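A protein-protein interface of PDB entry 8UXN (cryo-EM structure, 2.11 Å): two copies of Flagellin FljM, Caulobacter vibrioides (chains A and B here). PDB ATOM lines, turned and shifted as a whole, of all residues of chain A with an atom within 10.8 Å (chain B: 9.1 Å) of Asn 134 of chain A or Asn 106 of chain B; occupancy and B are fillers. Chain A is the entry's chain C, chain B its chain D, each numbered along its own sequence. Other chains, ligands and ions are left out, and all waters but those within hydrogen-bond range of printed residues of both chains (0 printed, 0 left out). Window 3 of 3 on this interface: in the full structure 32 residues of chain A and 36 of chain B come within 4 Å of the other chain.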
ATOM      1  N   ASP A  67      21.150   2.859 -23.147  1.00  0.00           N
ATOM      2  CA  ASP A  67      21.327   3.103 -21.720  1.00  0.00           C
ATOM      3  C   ASP A  67      22.569   3.944 -21.460  1.00  0.00           C
ATOM      4  O   ASP A  67      22.543   4.871 -20.645  1.00  0.00           O
ATOM      5  CB  ASP A  67      21.434   1.781 -20.971  1.00  0.00           C
ATOM      6  CG  ASP A  67      20.093   1.229 -20.548  1.00  0.00           C
ATOM      7  OD1 ASP A  67      20.073   0.206 -19.839  1.00  0.00           O
ATOM      8  OD2 ASP A  67      19.054   1.812 -20.916  1.00  0.00           O
ATOM      9  N   GLN A  70      22.006   7.627 -22.550  1.00  0.00           N
ATOM     10  CA  GLN A  70      21.167   8.317 -21.575  1.00  0.00           C
ATOM     11  C   GLN A  70      21.927   8.607 -20.288  1.00  0.00           C
ATOM     12  O   GLN A  70      21.741   9.663 -19.672  1.00  0.00           O
ATOM     13  CB  GLN A  70      19.919   7.493 -21.291  1.00  0.00           C
ATOM     14  CG  GLN A  70      18.937   7.505 -22.423  1.00  0.00           C
ATOM     15  CD  GLN A  70      17.798   6.549 -22.212  1.00  0.00           C
ATOM     16  OE1 GLN A  70      17.981   5.437 -21.732  1.00  0.00           O
ATOM     17  NE2 GLN A  70      16.607   6.988 -22.548  1.00  0.00           N
ATOM     18  N   ARG A  71      22.809   7.695 -19.886  1.00  0.00           N
ATOM     19  CA  ARG A  71      23.660   7.939 -18.730  1.00  0.00           C
ATOM     20  C   ARG A  71      24.558   9.146 -18.959  1.00  0.00           C
ATOM     21  O   ARG A  71      24.746   9.974 -18.060  1.00  0.00           O
ATOM     22  CB  ARG A  71      24.489   6.690 -18.456  1.00  0.00           C
ATOM     23  CG  ARG A  71      25.183   6.629 -17.134  1.00  0.00           C
ATOM     24  CD  ARG A  71      25.365   5.182 -16.691  1.00  0.00           C
ATOM     25  NE  ARG A  71      25.838   4.303 -17.754  1.00  0.00           N
ATOM     26  CZ  ARG A  71      25.168   3.259 -18.228  1.00  0.00           C
ATOM     27  NH1 ARG A  71      23.975   2.933 -17.765  1.00  0.00           N
ATOM     28  NH2 ARG A  71      25.710   2.523 -19.189  1.00  0.00           N
ATOM     29  N   GLY A  72      25.079   9.288 -20.176  1.00  0.00           N
ATOM     30  CA  GLY A  72      25.910  10.438 -20.472  1.00  0.00           C
ATOM     31  C   GLY A  72      25.133  11.736 -20.443  1.00  0.00           C
ATOM     32  O   GLY A  72      25.626  12.755 -19.950  1.00  0.00           O
ATOM     33  N   GLN A  73      23.898  11.710 -20.939  1.00  0.00           N
ATOM     34  CA  GLN A  73      23.070  12.908 -20.862  1.00  0.00           C
ATOM     35  C   GLN A  73      22.767  13.287 -19.412  1.00  0.00           C
ATOM     36  O   GLN A  73      22.781  14.469 -19.064  1.00  0.00           O
ATOM     37  CB  GLN A  73      21.784  12.707 -21.662  1.00  0.00           C
ATOM     38  CG  GLN A  73      21.968  12.911 -23.145  1.00  0.00           C
ATOM     39  CD  GLN A  73      20.705  12.669 -23.936  1.00  0.00           C
ATOM     40  OE1 GLN A  73      20.136  13.592 -24.495  1.00  0.00           O
ATOM     41  NE2 GLN A  73      20.267  11.429 -23.991  1.00  0.00           N
ATOM     42  N   SER A  74      22.561  12.297 -18.539  1.00  0.00           N
ATOM     43  CA  SER A  74      22.329  12.600 -17.124  1.00  0.00           C
ATOM     44  C   SER A  74      23.563  13.206 -16.460  1.00  0.00           C
ATOM     45  O   SER A  74      23.457  14.160 -15.673  1.00  0.00           O
ATOM     46  CB  SER A  74      21.916  11.341 -16.373  1.00  0.00           C
ATOM     47  OG  SER A  74      20.706  10.814 -16.852  1.00  0.00           O
ATOM     48  N   THR A  75      24.739  12.658 -16.764  1.00  0.00           N
ATOM     49  CA  THR A  75      25.976  13.187 -16.202  1.00  0.00           C
ATOM     50  C   THR A  75      26.199  14.632 -16.626  1.00  0.00           C
ATOM     51  O   THR A  75      26.537  15.493 -15.799  1.00  0.00           O
ATOM     52  CB  THR A  75      27.148  12.308 -16.642  1.00  0.00           C
ATOM     53  OG1 THR A  75      26.821  10.936 -16.419  1.00  0.00           O
ATOM     54  CG2 THR A  75      28.406  12.656 -15.892  1.00  0.00           C
ATOM     55  N   ILE A  76      25.969  14.927 -17.906  1.00  0.00           N
ATOM     56  CA  ILE A  76      26.112  16.301 -18.365  1.00  0.00           C
ATOM     57  C   ILE A  76      25.051  17.207 -17.744  1.00  0.00           C
ATOM     58  O   ILE A  76      25.323  18.375 -17.467  1.00  0.00           O
ATOM     59  CB  ILE A  76      26.087  16.351 -19.903  1.00  0.00           C
ATOM     60  CG1 ILE A  76      27.331  15.672 -20.476  1.00  0.00           C
ATOM     61  CG2 ILE A  76      25.969  17.781 -20.403  1.00  0.00           C
ATOM     62  CD1 ILE A  76      27.275  15.440 -21.940  1.00  0.00           C
ATOM     63  N   ASP A  77      23.845  16.693 -17.493  1.00  0.00           N
ATOM     64  CA  ASP A  77      22.820  17.508 -16.847  1.00  0.00           C
ATOM     65  C   ASP A  77      23.260  17.947 -15.459  1.00  0.00           C
ATOM     66  O   ASP A  77      23.074  19.109 -15.075  1.00  0.00           O
ATOM     67  CB  ASP A  77      21.508  16.731 -16.739  1.00  0.00           C
ATOM     68  CG  ASP A  77      20.625  16.884 -17.952  1.00  0.00           C
ATOM     69  OD1 ASP A  77      20.677  17.940 -18.612  1.00  0.00           O
ATOM     70  OD2 ASP A  77      19.855  15.947 -18.240  1.00  0.00           O
ATOM     71  N   VAL A  78      23.843  17.028 -14.690  1.00  0.00           N
ATOM     72  CA  VAL A  78      24.309  17.413 -13.362  1.00  0.00           C
ATOM     73  C   VAL A  78      25.439  18.434 -13.468  1.00  0.00           C
ATOM     74  O   VAL A  78      25.488  19.410 -12.704  1.00  0.00           O
ATOM     75  CB  VAL A  78      24.726  16.170 -12.554  1.00  0.00           C
ATOM     76  CG1 VAL A  78      25.294  16.578 -11.220  1.00  0.00           C
ATOM     77  CG2 VAL A  78      23.543  15.251 -12.360  1.00  0.00           C
ATOM     78  N   ALA A  79      26.327  18.263 -14.452  1.00  0.00           N
ATOM     79  CA  ALA A  79      27.384  19.254 -14.630  1.00  0.00           C
ATOM     80  C   ALA A  79      26.821  20.626 -14.986  1.00  0.00           C
ATOM     81  O   ALA A  79      27.321  21.643 -14.511  1.00  0.00           O
ATOM     82  CB  ALA A  79      28.369  18.799 -15.698  1.00  0.00           C
ATOM     83  N   SER A 129      32.763  20.128  -6.707  1.00  0.00           N
ATOM     84  CA  SER A 129      32.966  18.791  -6.174  1.00  0.00           C
ATOM     85  C   SER A 129      31.672  17.997  -6.098  1.00  0.00           C
ATOM     86  O   SER A 129      31.719  16.768  -6.132  1.00  0.00           O
ATOM     87  CB  SER A 129      33.623  18.851  -4.798  1.00  0.00           C
ATOM     88  OG  SER A 129      32.670  19.053  -3.782  1.00  0.00           O
ATOM     89  N   ASN A 130      30.526  18.657  -6.008  1.00  0.00           N
ATOM     90  CA  ASN A 130      29.277  17.915  -5.919  1.00  0.00           C
ATOM     91  C   ASN A 130      28.672  17.550  -7.273  1.00  0.00           C
ATOM     92  O   ASN A 130      27.602  16.944  -7.303  1.00  0.00           O
ATOM     93  CB  ASN A 130      28.268  18.696  -5.080  1.00  0.00           C
ATOM     94  CG  ASN A 130      28.407  18.406  -3.607  1.00  0.00           C
ATOM     95  OD1 ASN A 130      27.857  17.438  -3.106  1.00  0.00           O
ATOM     96  ND2 ASN A 130      29.158  19.235  -2.910  1.00  0.00           N
ATOM     97  N   ALA A 131      29.324  17.877  -8.384  1.00  0.00           N
ATOM     98  CA  ALA A 131      28.742  17.694  -9.714  1.00  0.00           C
ATOM     99  C   ALA A 131      28.913  16.260 -10.231  1.00  0.00           C
ATOM    100  O   ALA A 131      29.447  16.015 -11.305  1.00  0.00           O
ATOM    101  CB  ALA A 131      29.357  18.694 -10.679  1.00  0.00           C
ATOM    102  N   LYS A 132      28.414  15.305  -9.460  1.00  0.00           N
ATOM    103  CA  LYS A 132      28.574  13.890  -9.761  1.00  0.00           C
ATOM    104  C   LYS A 132      27.220  13.245 -10.011  1.00  0.00           C
ATOM    105  O   LYS A 132      26.243  13.555  -9.331  1.00  0.00           O
ATOM    106  CB  LYS A 132      29.288  13.165  -8.616  1.00  0.00           C
ATOM    107  CG  LYS A 132      30.703  13.640  -8.389  1.00  0.00           C
ATOM    108  CD  LYS A 132      31.457  12.797  -7.385  1.00  0.00           C
ATOM    109  CE  LYS A 132      30.560  12.253  -6.299  1.00  0.00           C
ATOM    110  NZ  LYS A 132      30.413  13.197  -5.156  1.00  0.00           N
ATOM    111  N   PHE A 133      27.164  12.345 -10.982  1.00  0.00           N
ATOM    112  CA  PHE A 133      25.981  11.533 -11.241  1.00  0.00           C
ATOM    113  C   PHE A 133      26.357  10.080 -11.007  1.00  0.00           C
ATOM    114  O   PHE A 133      27.070   9.484 -11.818  1.00  0.00           O
ATOM    115  CB  PHE A 133      25.447  11.742 -12.660  1.00  0.00           C
ATOM    116  CG  PHE A 133      24.210  10.948 -12.961  1.00  0.00           C
ATOM    117  CD1 PHE A 133      22.980  11.346 -12.475  1.00  0.00           C
ATOM    118  CD2 PHE A 133      24.278   9.795 -13.710  1.00  0.00           C
ATOM    119  CE1 PHE A 133      21.845  10.616 -12.739  1.00  0.00           C
ATOM    120  CE2 PHE A 133      23.138   9.059 -13.975  1.00  0.00           C
ATOM    121  CZ  PHE A 133      21.927   9.470 -13.488  1.00  0.00           C
ATOM    122  N   ASN A 134      25.892   9.519  -9.895  1.00  0.00           N
ATOM    123  CA  ASN A 134      26.171   8.132  -9.522  1.00  0.00           C
ATOM    124  C   ASN A 134      27.662   7.819  -9.576  1.00  0.00           C
ATOM    125  O   ASN A 134      28.099   6.858 -10.204  1.00  0.00           O
ATOM    126  CB  ASN A 134      25.383   7.159 -10.394  1.00  0.00           C
ATOM    127  CG  ASN A 134      23.915   7.211 -10.118  1.00  0.00           C
ATOM    128  OD1 ASN A 134      23.461   6.806  -9.054  1.00  0.00           O
ATOM    129  ND2 ASN A 134      23.158   7.728 -11.065  1.00  0.00           N
ATOM    130  N   GLY A 135      28.450   8.665  -8.932  1.00  0.00           N
ATOM    131  CA  GLY A 135      29.859   8.412  -8.763  1.00  0.00           C
ATOM    132  C   GLY A 135      30.754   8.840  -9.900  1.00  0.00           C
ATOM    133  O   GLY A 135      31.970   8.681  -9.791  1.00  0.00           O
ATOM    134  N   VAL A 136      30.211   9.390 -10.972  1.00  0.00           N
ATOM    135  CA  VAL A 136      31.029   9.837 -12.089  1.00  0.00           C
ATOM    136  C   VAL A 136      30.710  11.294 -12.379  1.00  0.00           C
ATOM    137  O   VAL A 136      29.583  11.756 -12.190  1.00  0.00           O
ATOM    138  CB  VAL A 136      30.828   8.951 -13.342  1.00  0.00           C
ATOM    139  CG1 VAL A 136      29.466   9.144 -13.946  1.00  0.00           C
ATOM    140  CG2 VAL A 136      31.873   9.248 -14.359  1.00  0.00           C
ATOM    141  N   SER A 137      31.720  12.025 -12.824  1.00  0.00           N
ATOM    142  CA  SER A 137      31.577  13.438 -13.108  1.00  0.00           C
ATOM    143  C   SER A 137      32.329  13.788 -14.380  1.00  0.00           C
ATOM    144  O   SER A 137      33.389  13.235 -14.665  1.00  0.00           O
ATOM    145  CB  SER A 137      32.089  14.285 -11.948  1.00  0.00           C
ATOM    146  OG  SER A 137      31.906  15.659 -12.198  1.00  0.00           O
ATOM    147  N   ILE A 138      31.755  14.709 -15.150  1.00  0.00           N
ATOM    148  CA  ILE A 138      32.425  15.286 -16.301  1.00  0.00           C
ATOM    149  C   ILE A 138      33.022  16.648 -15.990  1.00  0.00           C
ATOM    150  O   ILE A 138      33.690  17.231 -16.846  1.00  0.00           O
ATOM    151  CB  ILE A 138      31.455  15.361 -17.501  1.00  0.00           C
ATOM    152  CG1 ILE A 138      32.200  15.446 -18.833  1.00  0.00           C
ATOM    153  CG2 ILE A 138      30.521  16.533 -17.364  1.00  0.00           C
ATOM    154  CD1 ILE A 138      32.911  14.199 -19.219  1.00  0.00           C
ATOM    155  N   ASP A 140      34.210  17.662 -12.385  1.00  0.00           N
ATOM    156  CA  ASP A 140      34.905  17.807 -11.112  1.00  0.00           C
ATOM    157  C   ASP A 140      36.420  17.663 -11.225  1.00  0.00           C
ATOM    158  O   ASP A 140      37.112  17.778 -10.214  1.00  0.00           O
ATOM    159  CB  ASP A 140      34.345  16.820 -10.079  1.00  0.00           C
ATOM    160  CG  ASP A 140      34.732  15.383 -10.355  1.00  0.00           C
ATOM    161  OD1 ASP A 140      35.295  15.084 -11.424  1.00  0.00           O
ATOM    162  OD2 ASP A 140      34.445  14.533  -9.496  1.00  0.00           O
ATOM    163  N   THR A 142      38.254  14.965 -12.032  1.00  0.00           N
ATOM    164  CA  THR A 142      38.842  13.680 -11.677  1.00  0.00           C
ATOM    165  C   THR A 142      39.172  12.803 -12.879  1.00  0.00           C
ATOM    166  O   THR A 142      39.752  11.731 -12.694  1.00  0.00           O
ATOM    167  CB  THR A 142      37.918  12.921 -10.728  1.00  0.00           C
ATOM    168  OG1 THR A 142      36.663  12.671 -11.365  1.00  0.00           O
ATOM    169  CG2 THR A 142      37.686  13.724  -9.466  1.00  0.00           C
ATOM    170  N   LEU A 146      35.007  11.085 -20.437  1.00  0.00           N
ATOM    171  CA  LEU A 146      34.156   9.922 -20.287  1.00  0.00           C
ATOM    172  C   LEU A 146      33.812   9.404 -21.670  1.00  0.00           C
ATOM    173  O   LEU A 146      33.632  10.184 -22.605  1.00  0.00           O
ATOM    174  CB  LEU A 146      32.889  10.255 -19.504  1.00  0.00           C
ATOM    175  CG  LEU A 146      33.146  10.694 -18.066  1.00  0.00           C
ATOM    176  CD1 LEU A 146      31.871  11.153 -17.401  1.00  0.00           C
ATOM    177  CD2 LEU A 146      33.798   9.575 -17.295  1.00  0.00           C
ATOM    178  N   SER A 147      33.740   8.094 -21.802  1.00  0.00           N
ATOM    179  CA  SER A 147      33.420   7.470 -23.072  1.00  0.00           C
ATOM    180  C   SER A 147      32.155   6.647 -22.915  1.00  0.00           C
ATOM    181  O   SER A 147      32.102   5.726 -22.099  1.00  0.00           O
ATOM    182  CB  SER A 147      34.577   6.603 -23.563  1.00  0.00           C
ATOM    183  OG  SER A 147      35.034   5.752 -22.537  1.00  0.00           O
ATOM    184  N   PHE A 148      31.143   6.988 -23.694  1.00  0.00           N
ATOM    185  CA  PHE A 148      29.869   6.297 -23.700  1.00  0.00           C
ATOM    186  C   PHE A 148      29.765   5.468 -24.971  1.00  0.00           C
ATOM    187  O   PHE A 148      30.436   5.750 -25.963  1.00  0.00           O
ATOM    188  CB  PHE A 148      28.726   7.307 -23.579  1.00  0.00           C
ATOM    189  CG  PHE A 148      28.877   8.223 -22.405  1.00  0.00           C
ATOM    190  CD1 PHE A 148      28.513   7.809 -21.140  1.00  0.00           C
ATOM    191  CD2 PHE A 148      29.437   9.472 -22.553  1.00  0.00           C
ATOM    192  CE1 PHE A 148      28.680   8.627 -20.063  1.00  0.00           C
ATOM    193  CE2 PHE A 148      29.606  10.295 -21.470  1.00  0.00           C
ATOM    194  CZ  PHE A 148      29.227   9.874 -20.226  1.00  0.00           C
ATOM    195  N   ALA B  99      27.711  -3.338 -21.763  1.00  0.00           N
ATOM    196  CA  ALA B  99      27.412  -2.356 -20.732  1.00  0.00           C
ATOM    197  C   ALA B  99      28.591  -2.136 -19.793  1.00  0.00           C
ATOM    198  O   ALA B  99      28.824  -1.009 -19.355  1.00  0.00           O
ATOM    199  CB  ALA B  99      26.182  -2.786 -19.943  1.00  0.00           C
ATOM    200  N   ALA B 100      29.354  -3.183 -19.491  1.00  0.00           N
ATOM    201  CA  ALA B 100      30.457  -3.054 -18.550  1.00  0.00           C
ATOM    202  C   ALA B 100      31.662  -2.338 -19.139  1.00  0.00           C
ATOM    203  O   ALA B 100      32.510  -1.874 -18.382  1.00  0.00           O
ATOM    204  CB  ALA B 100      30.871  -4.424 -18.030  1.00  0.00           C
ATOM    205  N   ASP B 102      31.464   0.508 -20.688  1.00  0.00           N
ATOM    206  CA  ASP B 102      31.251   1.929 -20.453  1.00  0.00           C
ATOM    207  C   ASP B 102      31.982   2.364 -19.184  1.00  0.00           C
ATOM    208  O   ASP B 102      31.874   1.722 -18.139  1.00  0.00           O
ATOM    209  CB  ASP B 102      29.744   2.187 -20.360  1.00  0.00           C
ATOM    210  CG  ASP B 102      29.381   3.633 -20.088  1.00  0.00           C
ATOM    211  OD1 ASP B 102      30.254   4.516 -20.080  1.00  0.00           O
ATOM    212  OD2 ASP B 102      28.179   3.887 -19.892  1.00  0.00           O
ATOM    213  N   THR B 103      32.706   3.477 -19.265  1.00  0.00           N
ATOM    214  CA  THR B 103      33.495   3.944 -18.129  1.00  0.00           C
ATOM    215  C   THR B 103      32.740   4.901 -17.219  1.00  0.00           C
ATOM    216  O   THR B 103      33.275   5.294 -16.184  1.00  0.00           O
ATOM    217  CB  THR B 103      34.791   4.601 -18.601  1.00  0.00           C
ATOM    218  OG1 THR B 103      34.495   5.788 -19.343  1.00  0.00           O
ATOM    219  CG2 THR B 103      35.578   3.643 -19.468  1.00  0.00           C
ATOM    220  N   SER B 104      31.517   5.282 -17.565  1.00  0.00           N
ATOM    221  CA  SER B 104      30.716   6.084 -16.656  1.00  0.00           C
ATOM    222  C   SER B 104      30.080   5.257 -15.554  1.00  0.00           C
ATOM    223  O   SER B 104      29.472   5.830 -14.648  1.00  0.00           O
ATOM    224  CB  SER B 104      29.626   6.837 -17.416  1.00  0.00           C
ATOM    225  OG  SER B 104      28.629   5.961 -17.905  1.00  0.00           O
ATOM    226  N   LEU B 105      30.173   3.936 -15.624  1.00  0.00           N
ATOM    227  CA  LEU B 105      29.635   3.102 -14.563  1.00  0.00           C
ATOM    228  C   LEU B 105      30.445   3.270 -13.287  1.00  0.00           C
ATOM    229  O   LEU B 105      31.670   3.381 -13.324  1.00  0.00           O
ATOM    230  CB  LEU B 105      29.639   1.641 -14.988  1.00  0.00           C
ATOM    231  CG  LEU B 105      28.654   1.256 -16.080  1.00  0.00           C
ATOM    232  CD1 LEU B 105      28.501  -0.222 -16.070  1.00  0.00           C
ATOM    233  CD2 LEU B 105      27.319   1.929 -15.860  1.00  0.00           C
ATOM    234  N   ASN B 106      29.755   3.285 -12.157  1.00  0.00           N
ATOM    235  CA  ASN B 106      30.435   3.156 -10.883  1.00  0.00           C
ATOM    236  C   ASN B 106      30.752   1.688 -10.615  1.00  0.00           C
ATOM    237  O   ASN B 106      30.329   0.791 -11.344  1.00  0.00           O
ATOM    238  CB  ASN B 106      29.609   3.769  -9.753  1.00  0.00           C
ATOM    239  CG  ASN B 106      28.221   3.179  -9.636  1.00  0.00           C
ATOM    240  OD1 ASN B 106      28.029   1.974  -9.708  1.00  0.00           O
ATOM    241  ND2 ASN B 106      27.247   4.040  -9.429  1.00  0.00           N
ATOM    242  N   THR B 107      31.530   1.450  -9.561  1.00  0.00           N
ATOM    243  CA  THR B 107      32.033   0.107  -9.296  1.00  0.00           C
ATOM    244  C   THR B 107      30.909  -0.879  -8.993  1.00  0.00           C
ATOM    245  O   THR B 107      30.984  -2.045  -9.389  1.00  0.00           O
ATOM    246  CB  THR B 107      33.034   0.155  -8.140  1.00  0.00           C
ATOM    247  OG1 THR B 107      34.128   1.007  -8.490  1.00  0.00           O
ATOM    248  CG2 THR B 107      33.566  -1.224  -7.826  1.00  0.00           C
ATOM    249  N   ALA B 108      29.858  -0.437  -8.309  1.00  0.00           N
ATOM    250  CA  ALA B 108      28.786  -1.363  -7.960  1.00  0.00           C
ATOM    251  C   ALA B 108      28.035  -1.849  -9.198  1.00  0.00           C
ATOM    252  O   ALA B 108      27.711  -3.037  -9.308  1.00  0.00           O
ATOM    253  CB  ALA B 108      27.831  -0.707  -6.970  1.00  0.00           C
ATOM    254  N   SER B 109      27.789  -0.954 -10.154  1.00  0.00           N
ATOM    255  CA  SER B 109      27.124  -1.355 -11.388  1.00  0.00           C
ATOM    256  C   SER B 109      28.002  -2.286 -12.211  1.00  0.00           C
ATOM    257  O   SER B 109      27.515  -3.276 -12.775  1.00  0.00           O
ATOM    258  CB  SER B 109      26.753  -0.118 -12.198  1.00  0.00           C
ATOM    259  OG  SER B 109      25.966   0.765 -11.432  1.00  0.00           O
ATOM    260  N   PHE B 110      29.305  -2.005 -12.256  1.00  0.00           N
ATOM    261  CA  PHE B 110      30.217  -2.885 -12.969  1.00  0.00           C
ATOM    262  C   PHE B 110      30.225  -4.271 -12.346  1.00  0.00           C
ATOM    263  O   PHE B 110      30.183  -5.281 -13.058  1.00  0.00           O
ATOM    264  CB  PHE B 110      31.625  -2.286 -12.978  1.00  0.00           C
ATOM    265  CG  PHE B 110      32.650  -3.162 -13.630  1.00  0.00           C
ATOM    266  CD1 PHE B 110      33.292  -4.159 -12.917  1.00  0.00           C
ATOM    267  CD2 PHE B 110      32.966  -2.997 -14.959  1.00  0.00           C
ATOM    268  CE1 PHE B 110      34.215  -4.966 -13.518  1.00  0.00           C
ATOM    269  CE2 PHE B 110      33.896  -3.801 -15.561  1.00  0.00           C
ATOM    270  CZ  PHE B 110      34.519  -4.785 -14.843  1.00  0.00           C
ATOM    271  N   ASN B 111      30.244  -4.339 -11.018  1.00  0.00           N
ATOM    272  CA  ASN B 111      30.266  -5.633 -10.355  1.00  0.00           C
ATOM    273  C   ASN B 111      28.967  -6.394 -10.575  1.00  0.00           C
ATOM    274  O   ASN B 111      28.985  -7.618 -10.728  1.00  0.00           O
ATOM    275  CB  ASN B 111      30.532  -5.454  -8.865  1.00  0.00           C
ATOM    276  CG  ASN B 111      31.935  -4.984  -8.581  1.00  0.00           C
ATOM    277  OD1 ASN B 111      32.807  -5.045  -9.439  1.00  0.00           O
ATOM    278  ND2 ASN B 111      32.159  -4.513  -7.372  1.00  0.00           N
ATOM    279  N   ALA B 112      27.835  -5.690 -10.602  1.00  0.00           N
ATOM    280  CA  ALA B 112      26.572  -6.372 -10.850  1.00  0.00           C
ATOM    281  C   ALA B 112      26.537  -6.963 -12.252  1.00  0.00           C
ATOM    282  O   ALA B 112      26.085  -8.100 -12.446  1.00  0.00           O
ATOM    283  CB  ALA B 112      25.405  -5.408 -10.639  1.00  0.00           C
ATOM    284  N   LEU B 113      27.058  -6.224 -13.232  1.00  0.00           N
ATOM    285  CA  LEU B 113      27.121  -6.758 -14.584  1.00  0.00           C
ATOM    286  C   LEU B 113      28.045  -7.965 -14.664  1.00  0.00           C
ATOM    287  O   LEU B 113      27.723  -8.957 -15.327  1.00  0.00           O
ATOM    288  CB  LEU B 113      27.574  -5.672 -15.550  1.00  0.00           C
ATOM    289  CG  LEU B 113      26.561  -4.557 -15.771  1.00  0.00           C
ATOM    290  CD1 LEU B 113      27.225  -3.410 -16.451  1.00  0.00           C
ATOM    291  CD2 LEU B 113      25.384  -5.055 -16.587  1.00  0.00           C
ATOM    292  N   ALA B 180      36.907  -2.277 -17.297  1.00  0.00           N
ATOM    293  CA  ALA B 180      36.160  -1.859 -18.472  1.00  0.00           C
ATOM    294  C   ALA B 180      36.883  -2.226 -19.761  1.00  0.00           C
ATOM    295  O   ALA B 180      36.235  -2.559 -20.758  1.00  0.00           O
ATOM    296  CB  ALA B 180      35.892  -0.357 -18.415  1.00  0.00           C
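Gln 70 of chain A touches none of the printed residues of chain B. Of the printed residues of chain B, Arg 71 of chain A touches Asp 102 (2.9 Å), Ser 104 (3.2 Å) and Leu 105 (3.4 Å). No residue of chain B comes within 4 Å of Phe 133 of chain A. Asn 134 of chain A touches just one residue of chain B: Asn 106 (3.0 Å). No residue of chain B comes within 4 Å of Gly 135 of chain A. Of the printed residues of chain B, Val 136 of chain A touches Ser 104 (3.4 Å). Of the printed residues of chain B, Ser 147 of chain A touches Asp 102 and Thr 103. Of the printed residues of chain B, Phe 148 of chain A touches Asp 102 (3.9 Å) and Ser 104 (3.3 Å). Ala 99 of chain B touches none of the printed residues of chain A. Of the printed residues of chain A, Thr 103 of chain B touches Ser 147 (3.2 Å). Leu 105 of chain B touches just one residue of chain A: Arg 71 (3.4 Å). Asn 106 of chain B touches one residue of chain A. No residue of chain A comes within 4 Å of Thr 107 of chain B. Ala 108 of chain B touches none of the printed residues of chain A. No residue of chain A comes within 4 Å of Ser 109 of chain B. The nearest residue of chain B that does not touch Asn 134 of chain A is Ser 104 of chain B (4.8 Å). The nearest printed residue of chain A that does not touch Asp 102 of chain B is Asp 67 of chain A (5.8 Å).
No position is printed for both chains.
The guanidinium group (NH2) of Arg 71 of chain A lies within salt-bridge range of the side-chain carboxylate (OD2) of Asp 102 of chain B (2.9 Å). NE of Arg 71 of chain A lies within hydrogen-bond range of OG of Ser 104 of chain B (3.2 Å). ND2 of Asn 106 of chain B is in hydrogen-bond range of O of Asn 134 of chain A, 3.0 Å away. The side-chain hydroxyl (OG) of Ser 147 of chain A is in hydrogen-bond range of the side-chain hydroxyl (OG1) of Thr 103 of chain B, 3.2 Å away. O of Ser 147 of chain A sits close to OD1 of Asp 102 of chain B (3.0 Å).
Leu 105 of chain B touches Arg 71 of chain A. Val 136 of chain A touches Ser 104 of chain B. Asp 102 of chain B touches Phe 148 of chain A. Ser 104 of chain B touches Phe 148 of chain A (CB to CE1, 3.3 Å).
The backbone carbonyl oxygen (O) of Arg 71 of chain A is in hydrogen-bond range of the side-chain hydroxyl (OG1) of Thr 75 of chain A, 2.8 Å away. The side-chain carboxylate (OD2) of Asp 102 of chain B sits at hydrogen-bond distance from the side-chain hydroxyl (OG) of Ser 104 of chain B (2.9 Å). OD1 of Asn 106 of chain B sits close to N of Ala 108 of chain B (3.3 Å). OD1 of Asn 106 of chain B is in hydrogen-bond range of OG of Ser 109 of chain B.
Of the 26 printed residues of chain A, 5 touch a printed residue of chain B. Hydrophobic or aromatic side chains of chain A within 4 Å of the printed part of chain B: Val 136 and Phe 148. Along chain A the printed residues that touch a printed residue of chain B span positions 71 to 148. Among the printed residues, 9 pairs touch across the chains. Among the printed residues, Asp or Glu carboxylates within 4 Å of a Lys or Arg side-chain nitrogen of the other chain: Arg 71 of chain A with Asp 102 of chain B (2.9 Å).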
